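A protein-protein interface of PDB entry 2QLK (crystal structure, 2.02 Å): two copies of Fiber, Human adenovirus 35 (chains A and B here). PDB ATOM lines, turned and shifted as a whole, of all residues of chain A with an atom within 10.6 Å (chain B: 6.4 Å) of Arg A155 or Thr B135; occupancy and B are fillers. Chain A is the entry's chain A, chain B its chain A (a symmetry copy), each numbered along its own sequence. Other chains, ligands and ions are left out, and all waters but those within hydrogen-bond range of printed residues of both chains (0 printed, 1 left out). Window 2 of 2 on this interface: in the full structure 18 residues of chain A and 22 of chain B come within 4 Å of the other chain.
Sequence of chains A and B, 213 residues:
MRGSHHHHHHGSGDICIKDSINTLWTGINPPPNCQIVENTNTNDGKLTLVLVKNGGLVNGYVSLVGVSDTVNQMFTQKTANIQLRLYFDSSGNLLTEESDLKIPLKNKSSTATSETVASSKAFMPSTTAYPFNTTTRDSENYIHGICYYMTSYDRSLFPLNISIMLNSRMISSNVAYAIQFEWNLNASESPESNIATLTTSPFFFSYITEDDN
Among the printed residues, pairs that only touch across the chains: Met A150 with Tyr B142 and Thr A199 with Ser B139.
NH2 of Arg A155 lies within hydrogen-bond range of O of Thr B135 (3.0 Å).
The guanidinium group (NH1) of Arg A155 sits at hydrogen-bond distance from the side-chain hydroxyl (OG) of Ser B139 (3.0 Å).
Of the printed residues of chain B, Met A150 touches Tyr B142.
Of the printed residues of chain B, Thr A199 touches Ser B139 (3.8 Å).
Thr B134 touches none of the printed residues of chain A.
Thr B135 touches just one residue of chain A: Arg A155 (3.0 Å).
No residue of chain A comes within 4 Å of Thr B136.
No residue of chain A comes within 4 Å of Asp B138.
Of the printed residues of chain A, Ser B139 touches Arg A155 and Thr A199.
Of the printed residues of chain A, Tyr B142 touches Met A150.
The nearest residue of chain B that does not touch Arg A155 is Asp B138 (4.5 Å).
The nearest residue of chain A that does not touch Thr B135 is Ser A152 (7.1 Å).
Hydrophobic or aromatic side chains of chain A that line the printed part of chain B: Met A150.
Of the 10 printed residues of chain B, 3 touch a printed residue of chain A.
Hydrophobic or aromatic side chains of chain B within 4 Å of the printed part of chain A: Tyr B142.
Among the printed residues, no Asp or Glu carboxylate lies within 4 Å of a Lys or Arg side-chain nitrogen of the other chain.
N of Arg A155 is in hydrogen-bond range of OG1 of Thr A151, at 3.1 Å.
The side-chain hydroxyl (OG1) of Thr B135 is in hydrogen-bond range of the guanidinium group (NH1) of Arg B169, 3.4 Å away.
The side-chain carboxylate of Asp B138 sits close to the side-chain hydroxyl of Tyr B142, at 3.2 Å.
No position is printed for both chains.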
ATOM      1  N   TYR A 148      13.383 -16.429  -2.762  1.00  0.00           N
ATOM      2  CA  TYR A 148      14.671 -17.056  -2.975  1.00  0.00           C
ATOM      3  C   TYR A 148      15.077 -18.234  -2.139  1.00  0.00           C
ATOM      4  O   TYR A 148      14.584 -18.458  -1.037  1.00  0.00           O
ATOM      5  CB  TYR A 148      15.781 -15.995  -2.831  1.00  0.00           C
ATOM      6  CG  TYR A 148      15.570 -14.755  -3.653  1.00  0.00           C
ATOM      7  CD1 TYR A 148      14.612 -13.797  -3.275  1.00  0.00           C
ATOM      8  CD2 TYR A 148      16.249 -14.578  -4.865  1.00  0.00           C
ATOM      9  CE1 TYR A 148      14.329 -12.717  -4.086  1.00  0.00           C
ATOM     10  CE2 TYR A 148      15.972 -13.506  -5.687  1.00  0.00           C
ATOM     11  CZ  TYR A 148      15.013 -12.582  -5.300  1.00  0.00           C
ATOM     12  OH  TYR A 148      14.715 -11.524  -6.119  1.00  0.00           O
ATOM     13  N   TYR A 149      16.024 -18.983  -2.686  1.00  0.00           N
ATOM     14  CA  TYR A 149      16.614 -20.116  -1.997  1.00  0.00           C
ATOM     15  C   TYR A 149      18.101 -19.765  -1.859  1.00  0.00           C
ATOM     16  O   TYR A 149      18.755 -19.386  -2.834  1.00  0.00           O
ATOM     17  CB  TYR A 149      16.507 -21.402  -2.816  1.00  0.00           C
ATOM     18  CG  TYR A 149      17.238 -22.540  -2.148  1.00  0.00           C
ATOM     19  CD1 TYR A 149      16.804 -23.023  -0.922  1.00  0.00           C
ATOM     20  CD2 TYR A 149      18.396 -23.089  -2.705  1.00  0.00           C
ATOM     21  CE1 TYR A 149      17.495 -24.021  -0.248  1.00  0.00           C
ATOM     22  CE2 TYR A 149      19.110 -24.115  -2.034  1.00  0.00           C
ATOM     23  CZ  TYR A 149      18.640 -24.568  -0.804  1.00  0.00           C
ATOM     24  OH  TYR A 149      19.276 -25.589  -0.118  1.00  0.00           O
ATOM     25  N   MET A 150      18.612 -19.900  -0.645  1.00  0.00           N
ATOM     26  CA  MET A 150      20.011 -19.643  -0.312  1.00  0.00           C
ATOM     27  C   MET A 150      20.725 -21.012  -0.248  1.00  0.00           C
ATOM     28  O   MET A 150      20.358 -21.882   0.557  1.00  0.00           O
ATOM     29  CB  MET A 150      20.059 -18.928   1.046  1.00  0.00           C
ATOM     30  CG  MET A 150      21.419 -18.483   1.528  1.00  0.00           C
ATOM     31  SD  MET A 150      21.226 -17.286   2.893  1.00  0.00           S
ATOM     32  CE  MET A 150      21.713 -15.821   2.068  1.00  0.00           C
ATOM     33  N   THR A 151      21.719 -21.221  -1.105  1.00  0.00           N
ATOM     34  CA  THR A 151      22.429 -22.513  -1.126  1.00  0.00           C
ATOM     35  C   THR A 151      23.207 -22.717   0.157  1.00  0.00           C
ATOM     36  O   THR A 151      23.669 -21.763   0.783  1.00  0.00           O
ATOM     37  CB  THR A 151      23.411 -22.625  -2.295  1.00  0.00           C
ATOM     38  OG1 THR A 151      24.607 -21.898  -1.993  1.00  0.00           O
ATOM     39  CG2 THR A 151      22.782 -22.055  -3.548  1.00  0.00           C
ATOM     40  N   SER A 152      23.342 -23.981   0.526  1.00  0.00           N
ATOM     41  CA  SER A 152      24.010 -24.392   1.738  1.00  0.00           C
ATOM     42  C   SER A 152      25.527 -24.252   1.696  1.00  0.00           C
ATOM     43  O   SER A 152      26.162 -24.227   2.740  1.00  0.00           O
ATOM     44  CB  SER A 152      23.666 -25.848   2.029  1.00  0.00           C
ATOM     45  OG  SER A 152      24.215 -26.671   1.013  1.00  0.00           O
ATOM     46  N   TYR A 153      26.119 -24.168   0.512  1.00  0.00           N
ATOM     47  CA  TYR A 153      27.575 -24.068   0.453  1.00  0.00           C
ATOM     48  C   TYR A 153      28.151 -22.659   0.331  1.00  0.00           C
ATOM     49  O   TYR A 153      28.813 -22.180   1.249  1.00  0.00           O
ATOM     50  CB  TYR A 153      28.129 -24.969  -0.664  1.00  0.00           C
ATOM     51  CG  TYR A 153      27.386 -24.916  -1.983  1.00  0.00           C
ATOM     52  CD1 TYR A 153      27.393 -23.769  -2.767  1.00  0.00           C
ATOM     53  CD2 TYR A 153      26.696 -26.031  -2.460  1.00  0.00           C
ATOM     54  CE1 TYR A 153      26.737 -23.728  -3.993  1.00  0.00           C
ATOM     55  CE2 TYR A 153      26.037 -26.001  -3.687  1.00  0.00           C
ATOM     56  CZ  TYR A 153      26.065 -24.843  -4.448  1.00  0.00           C
ATOM     57  OH  TYR A 153      25.437 -24.796  -5.672  1.00  0.00           O
ATOM     58  N   ASP A 154      27.898 -21.996  -0.792  1.00  0.00           N
ATOM     59  CA  ASP A 154      28.418 -20.654  -1.007  1.00  0.00           C
ATOM     60  C   ASP A 154      27.378 -19.601  -0.689  1.00  0.00           C
ATOM     61  O   ASP A 154      27.593 -18.421  -0.953  1.00  0.00           O
ATOM     62  CB  ASP A 154      28.893 -20.477  -2.455  1.00  0.00           C
ATOM     63  CG  ASP A 154      27.802 -20.763  -3.473  1.00  0.00           C
ATOM     64  OD1 ASP A 154      26.627 -20.416  -3.227  1.00  0.00           O
ATOM     65  OD2 ASP A 154      28.121 -21.327  -4.535  1.00  0.00           O
ATOM     66  N   ARG A 155      26.246 -20.038  -0.140  1.00  0.00           N
ATOM     67  CA  ARG A 155      25.158 -19.145   0.247  1.00  0.00           C
ATOM     68  C   ARG A 155      24.663 -18.249  -0.868  1.00  0.00           C
ATOM     69  O   ARG A 155      24.243 -17.123  -0.618  1.00  0.00           O
ATOM     70  CB  ARG A 155      25.561 -18.258   1.433  1.00  0.00           C
ATOM     71  CG  ARG A 155      25.776 -18.974   2.761  1.00  0.00           C
ATOM     72  CD  ARG A 155      24.562 -19.769   3.233  1.00  0.00           C
ATOM     73  NE  ARG A 155      24.757 -20.240   4.609  1.00  0.00           N
ATOM     74  CZ  ARG A 155      23.950 -21.082   5.254  1.00  0.00           C
ATOM     75  NH1 ARG A 155      22.869 -21.572   4.657  1.00  0.00           N
ATOM     76  NH2 ARG A 155      24.228 -21.430   6.506  1.00  0.00           N
ATOM     77  N   SER A 156      24.711 -18.724  -2.102  1.00  0.00           N
ATOM     78  CA  SER A 156      24.214 -17.910  -3.187  1.00  0.00           C
ATOM     79  C   SER A 156      22.690 -18.046  -3.259  1.00  0.00           C
ATOM     80  O   SER A 156      22.104 -19.002  -2.745  1.00  0.00           O
ATOM     81  CB  SER A 156      24.870 -18.311  -4.508  1.00  0.00           C
ATOM     82  OG  SER A 156      24.667 -19.672  -4.804  1.00  0.00           O
ATOM     83  N   LEU A 157      22.066 -17.061  -3.886  1.00  0.00           N
ATOM     84  CA  LEU A 157      20.628 -17.008  -4.026  1.00  0.00           C
ATOM     85  C   LEU A 157      20.096 -17.468  -5.356  1.00  0.00           C
ATOM     86  O   LEU A 157      20.539 -17.028  -6.427  1.00  0.00           O
ATOM     87  CB  LEU A 157      20.124 -15.587  -3.783  1.00  0.00           C
ATOM     88  CG  LEU A 157      20.323 -15.040  -2.368  1.00  0.00           C
ATOM     89  CD1 LEU A 157      19.712 -13.648  -2.258  1.00  0.00           C
ATOM     90  CD2 LEU A 157      19.671 -15.984  -1.376  1.00  0.00           C
ATOM     91  N   PHE A 158      19.145 -18.380  -5.293  1.00  0.00           N
ATOM     92  CA  PHE A 158      18.508 -18.832  -6.513  1.00  0.00           C
ATOM     93  C   PHE A 158      17.083 -18.295  -6.464  1.00  0.00           C
ATOM     94  O   PHE A 158      16.372 -18.511  -5.484  1.00  0.00           O
ATOM     95  CB  PHE A 158      18.486 -20.364  -6.581  1.00  0.00           C
ATOM     96  CG  PHE A 158      19.761 -20.974  -7.101  1.00  0.00           C
ATOM     97  CD1 PHE A 158      20.931 -20.927  -6.354  1.00  0.00           C
ATOM     98  CD2 PHE A 158      19.775 -21.629  -8.339  1.00  0.00           C
ATOM     99  CE1 PHE A 158      22.106 -21.531  -6.822  1.00  0.00           C
ATOM    100  CE2 PHE A 158      20.952 -22.244  -8.820  1.00  0.00           C
ATOM    101  CZ  PHE A 158      22.118 -22.195  -8.056  1.00  0.00           C
ATOM    102  N   PRO A 159      16.649 -17.578  -7.513  1.00  0.00           N
ATOM    103  CA  PRO A 159      15.279 -17.080  -7.458  1.00  0.00           C
ATOM    104  C   PRO A 159      14.282 -18.222  -7.673  1.00  0.00           C
ATOM    105  O   PRO A 159      14.548 -19.193  -8.400  1.00  0.00           O
ATOM    106  CB  PRO A 159      15.235 -16.038  -8.590  1.00  0.00           C
ATOM    107  CG  PRO A 159      16.229 -16.593  -9.580  1.00  0.00           C
ATOM    108  CD  PRO A 159      17.360 -17.037  -8.685  1.00  0.00           C
ATOM    109  N   PRO A 191      21.089 -26.011  -7.671  1.00  0.00           N
ATOM    110  CA  PRO A 191      21.601 -25.262  -6.518  1.00  0.00           C
ATOM    111  C   PRO A 191      22.384 -26.096  -5.503  1.00  0.00           C
ATOM    112  O   PRO A 191      23.285 -25.578  -4.851  1.00  0.00           O
ATOM    113  CB  PRO A 191      20.341 -24.603  -5.933  1.00  0.00           C
ATOM    114  CG  PRO A 191      19.215 -25.398  -6.458  1.00  0.00           C
ATOM    115  CD  PRO A 191      19.641 -25.812  -7.841  1.00  0.00           C
ATOM    116  N   GLU A 192      22.057 -27.380  -5.366  1.00  0.00           N
ATOM    117  CA  GLU A 192      22.782 -28.223  -4.418  1.00  0.00           C
ATOM    118  C   GLU A 192      23.267 -29.529  -5.046  1.00  0.00           C
ATOM    119  O   GLU A 192      22.676 -30.029  -5.991  1.00  0.00           O
ATOM    120  CB  GLU A 192      21.904 -28.559  -3.214  1.00  0.00           C
ATOM    121  CG  GLU A 192      21.358 -27.353  -2.475  1.00  0.00           C
ATOM    122  CD  GLU A 192      22.250 -26.895  -1.325  1.00  0.00           C
ATOM    123  OE1 GLU A 192      23.322 -27.510  -1.097  1.00  0.00           O
ATOM    124  OE2 GLU A 192      21.864 -25.918  -0.647  1.00  0.00           O
ATOM    125  N   ILE A 195      21.830 -33.488  -0.196  1.00  0.00           N
ATOM    126  CA  ILE A 195      20.842 -33.125   0.804  1.00  0.00           C
ATOM    127  C   ILE A 195      21.226 -31.854   1.539  1.00  0.00           C
ATOM    128  O   ILE A 195      22.374 -31.694   1.977  1.00  0.00           O
ATOM    129  CB  ILE A 195      20.658 -34.249   1.837  1.00  0.00           C
ATOM    130  CG1 ILE A 195      20.407 -35.575   1.120  1.00  0.00           C
ATOM    131  CG2 ILE A 195      19.494 -33.928   2.740  1.00  0.00           C
ATOM    132  CD1 ILE A 195      19.228 -35.543   0.149  1.00  0.00           C
ATOM    133  N   ALA A 196      20.251 -30.955   1.666  1.00  0.00           N
ATOM    134  CA  ALA A 196      20.430 -29.670   2.343  1.00  0.00           C
ATOM    135  C   ALA A 196      19.024 -29.214   2.662  1.00  0.00           C
ATOM    136  O   ALA A 196      18.119 -29.421   1.855  1.00  0.00           O
ATOM    137  CB  ALA A 196      21.106 -28.674   1.411  1.00  0.00           C
ATOM    138  N   THR A 197      18.826 -28.604   3.827  1.00  0.00           N
ATOM    139  CA  THR A 197      17.490 -28.173   4.223  1.00  0.00           C
ATOM    140  C   THR A 197      16.898 -27.228   3.209  1.00  0.00           C
ATOM    141  O   THR A 197      17.431 -26.134   2.963  1.00  0.00           O
ATOM    142  CB  THR A 197      17.477 -27.458   5.585  1.00  0.00           C
ATOM    143  OG1 THR A 197      18.165 -28.253   6.557  1.00  0.00           O
ATOM    144  CG2 THR A 197      16.053 -27.264   6.052  1.00  0.00           C
ATOM    145  N   LEU A 198      15.792 -27.647   2.608  1.00  0.00           N
ATOM    146  CA  LEU A 198      15.158 -26.793   1.626  1.00  0.00           C
ATOM    147  C   LEU A 198      14.492 -25.670   2.412  1.00  0.00           C
ATOM    148  O   LEU A 198      13.873 -25.935   3.426  1.00  0.00           O
ATOM    149  CB  LEU A 198      14.131 -27.583   0.807  1.00  0.00           C
ATOM    150  CG  LEU A 198      13.259 -26.769  -0.162  1.00  0.00           C
ATOM    151  CD1 LEU A 198      12.748 -27.668  -1.277  1.00  0.00           C
ATOM    152  CD2 LEU A 198      12.073 -26.125   0.601  1.00  0.00           C
ATOM    153  N   THR A 199      14.677 -24.422   1.979  1.00  0.00           N
ATOM    154  CA  THR A 199      14.031 -23.277   2.627  1.00  0.00           C
ATOM    155  C   THR A 199      13.673 -22.260   1.551  1.00  0.00           C
ATOM    156  O   THR A 199      14.434 -22.072   0.595  1.00  0.00           O
ATOM    157  CB  THR A 199      14.949 -22.567   3.640  1.00  0.00           C
ATOM    158  OG1 THR A 199      16.090 -22.047   2.946  1.00  0.00           O
ATOM    159  CG2 THR A 199      15.421 -23.536   4.714  1.00  0.00           C
ATOM    160  N   PHE B 132      18.922 -16.917  17.238  1.00  0.00           N
ATOM    161  CA  PHE B 132      20.308 -16.454  17.271  1.00  0.00           C
ATOM    162  C   PHE B 132      21.277 -17.627  17.154  1.00  0.00           C
ATOM    163  O   PHE B 132      20.862 -18.778  17.027  1.00  0.00           O
ATOM    164  CB  PHE B 132      20.577 -15.732  18.592  1.00  0.00           C
ATOM    165  CG  PHE B 132      20.323 -14.260  18.545  1.00  0.00           C
ATOM    166  CD1 PHE B 132      21.166 -13.424  17.822  1.00  0.00           C
ATOM    167  CD2 PHE B 132      19.262 -13.706  19.233  1.00  0.00           C
ATOM    168  CE1 PHE B 132      20.952 -12.052  17.791  1.00  0.00           C
ATOM    169  CE2 PHE B 132      19.033 -12.325  19.214  1.00  0.00           C
ATOM    170  CZ  PHE B 132      19.874 -11.500  18.496  1.00  0.00           C
ATOM    171  N   ASN B 133      22.571 -17.320  17.213  1.00  0.00           N
ATOM    172  CA  ASN B 133      23.636 -18.324  17.151  1.00  0.00           C
ATOM    173  C   ASN B 133      23.294 -19.615  16.409  1.00  0.00           C
ATOM    174  O   ASN B 133      23.424 -20.706  16.967  1.00  0.00           O
ATOM    175  CB  ASN B 133      24.092 -18.673  18.575  1.00  0.00           C
ATOM    176  CG  ASN B 133      24.888 -17.555  19.229  1.00  0.00           C
ATOM    177  OD1 ASN B 133      26.029 -17.282  18.842  1.00  0.00           O
ATOM    178  ND2 ASN B 133      24.290 -16.899  20.220  1.00  0.00           N
ATOM    179  N   THR B 134      22.868 -19.490  15.154  1.00  0.00           N
ATOM    180  CA  THR B 134      22.519 -20.656  14.339  1.00  0.00           C
ATOM    181  C   THR B 134      22.784 -20.453  12.849  1.00  0.00           C
ATOM    182  O   THR B 134      22.153 -19.609  12.209  1.00  0.00           O
ATOM    183  CB  THR B 134      21.022 -21.042  14.486  1.00  0.00           C
ATOM    184  OG1 THR B 134      20.207 -19.875  14.300  1.00  0.00           O
ATOM    185  CG2 THR B 134      20.748 -21.666  15.850  1.00  0.00           C
ATOM    186  N   THR B 135      23.719 -21.223  12.302  1.00  0.00           N
ATOM    187  CA  THR B 135      24.022 -21.150  10.877  1.00  0.00           C
ATOM    188  C   THR B 135      23.319 -22.350  10.250  1.00  0.00           C
ATOM    189  O   THR B 135      23.066 -22.385   9.044  1.00  0.00           O
ATOM    190  CB  THR B 135      25.534 -21.238  10.596  1.00  0.00           C
ATOM    191  OG1 THR B 135      26.215 -20.186  11.291  1.00  0.00           O
ATOM    192  CG2 THR B 135      25.803 -21.092   9.102  1.00  0.00           C
ATOM    193  N   THR B 136      23.013 -23.335  11.095  1.00  0.00           N
ATOM    194  CA  THR B 136      22.308 -24.540  10.674  1.00  0.00           C
ATOM    195  C   THR B 136      20.897 -24.053  10.391  1.00  0.00           C
ATOM    196  O   THR B 136      20.158 -24.629   9.588  1.00  0.00           O
ATOM    197  CB  THR B 136      22.250 -25.594  11.810  1.00  0.00           C
ATOM    198  OG1 THR B 136      23.578 -25.891  12.264  1.00  0.00           O
ATOM    199  CG2 THR B 136      21.593 -26.879  11.316  1.00  0.00           C
ATOM    200  N   ARG B 137      20.544 -22.973  11.079  1.00  0.00           N
ATOM    201  CA  ARG B 137      19.246 -22.332  10.948  1.00  0.00           C
ATOM    202  C   ARG B 137      19.470 -20.825  10.867  1.00  0.00           C
ATOM    203  O   ARG B 137      19.062 -20.071  11.752  1.00  0.00           O
ATOM    204  CB  ARG B 137      18.360 -22.670  12.148  1.00  0.00           C
ATOM    205  CG  ARG B 137      17.899 -24.120  12.201  1.00  0.00           C
ATOM    206  CD  ARG B 137      16.973 -24.324  13.380  1.00  0.00           C
ATOM    207  NE  ARG B 137      15.882 -23.352  13.387  1.00  0.00           N
ATOM    208  CZ  ARG B 137      14.981 -23.251  14.359  1.00  0.00           C
ATOM    209  NH1 ARG B 137      15.044 -24.065  15.408  1.00  0.00           N
ATOM    210  NH2 ARG B 137      14.014 -22.345  14.285  1.00  0.00           N
ATOM    211  N   ASP B 138      20.137 -20.405   9.796  1.00  0.00           N
ATOM    212  CA  ASP B 138      20.441 -19.001   9.557  1.00  0.00           C
ATOM    213  C   ASP B 138      19.695 -18.562   8.298  1.00  0.00           C
ATOM    214  O   ASP B 138      19.360 -17.385   8.134  1.00  0.00           O
ATOM    215  CB  ASP B 138      21.951 -18.828   9.362  1.00  0.00           C
ATOM    216  CG  ASP B 138      22.379 -17.374   9.341  1.00  0.00           C
ATOM    217  OD1 ASP B 138      22.142 -16.676  10.350  1.00  0.00           O
ATOM    218  OD2 ASP B 138      22.956 -16.933   8.320  1.00  0.00           O
ATOM    219  N   SER B 139      19.431 -19.530   7.420  1.00  0.00           N
ATOM    220  CA  SER B 139      18.728 -19.285   6.162  1.00  0.00           C
ATOM    221  C   SER B 139      17.337 -18.689   6.359  1.00  0.00           C
ATOM    222  O   SER B 139      16.955 -17.762   5.644  1.00  0.00           O
ATOM    223  CB  SER B 139      18.619 -20.584   5.352  1.00  0.00           C
ATOM    224  OG  SER B 139      19.897 -21.034   4.929  1.00  0.00           O
ATOM    225  N   TYR B 142      16.711 -14.738   6.855  1.00  0.00           N
ATOM    226  CA  TYR B 142      16.879 -13.731   5.817  1.00  0.00           C
ATOM    227  C   TYR B 142      15.621 -13.436   5.012  1.00  0.00           C
ATOM    228  O   TYR B 142      14.792 -14.333   4.765  1.00  0.00           O
ATOM    229  CB  TYR B 142      17.959 -14.172   4.825  1.00  0.00           C
ATOM    230  CG  TYR B 142      19.378 -14.150   5.355  1.00  0.00           C
ATOM    231  CD1 TYR B 142      20.085 -12.951   5.475  1.00  0.00           C
ATOM    232  CD2 TYR B 142      20.023 -15.332   5.724  1.00  0.00           C
ATOM    233  CE1 TYR B 142      21.408 -12.936   5.948  1.00  0.00           C
ATOM    234  CE2 TYR B 142      21.331 -15.329   6.193  1.00  0.00           C
ATOM    235  CZ  TYR B 142      22.022 -14.130   6.301  1.00  0.00           C
ATOM    236  OH  TYR B 142      23.334 -14.137   6.740  1.00  0.00           O
ATOM    237  N   ARG B 169      22.998 -12.933  14.500  1.00  0.00           N
ATOM    238  CA  ARG B 169      24.309 -12.581  15.058  1.00  0.00           C
ATOM    239  C   ARG B 169      24.229 -11.433  16.072  1.00  0.00           C
ATOM    240  O   ARG B 169      24.189 -10.266  15.683  1.00  0.00           O
ATOM    241  CB  ARG B 169      25.281 -12.167  13.945  1.00  0.00           C
ATOM    242  CG  ARG B 169      25.235 -12.990  12.657  1.00  0.00           C
ATOM    243  CD  ARG B 169      25.706 -14.423  12.827  1.00  0.00           C
ATOM    244  NE  ARG B 169      24.716 -15.253  13.504  1.00  0.00           N
ATOM    245  CZ  ARG B 169      24.741 -16.583  13.522  1.00  0.00           C
ATOM    246  NH1 ARG B 169      25.709 -17.239  12.894  1.00  0.00           N
ATOM    247  NH2 ARG B 169      23.797 -17.258  14.164  1.00  0.00           N
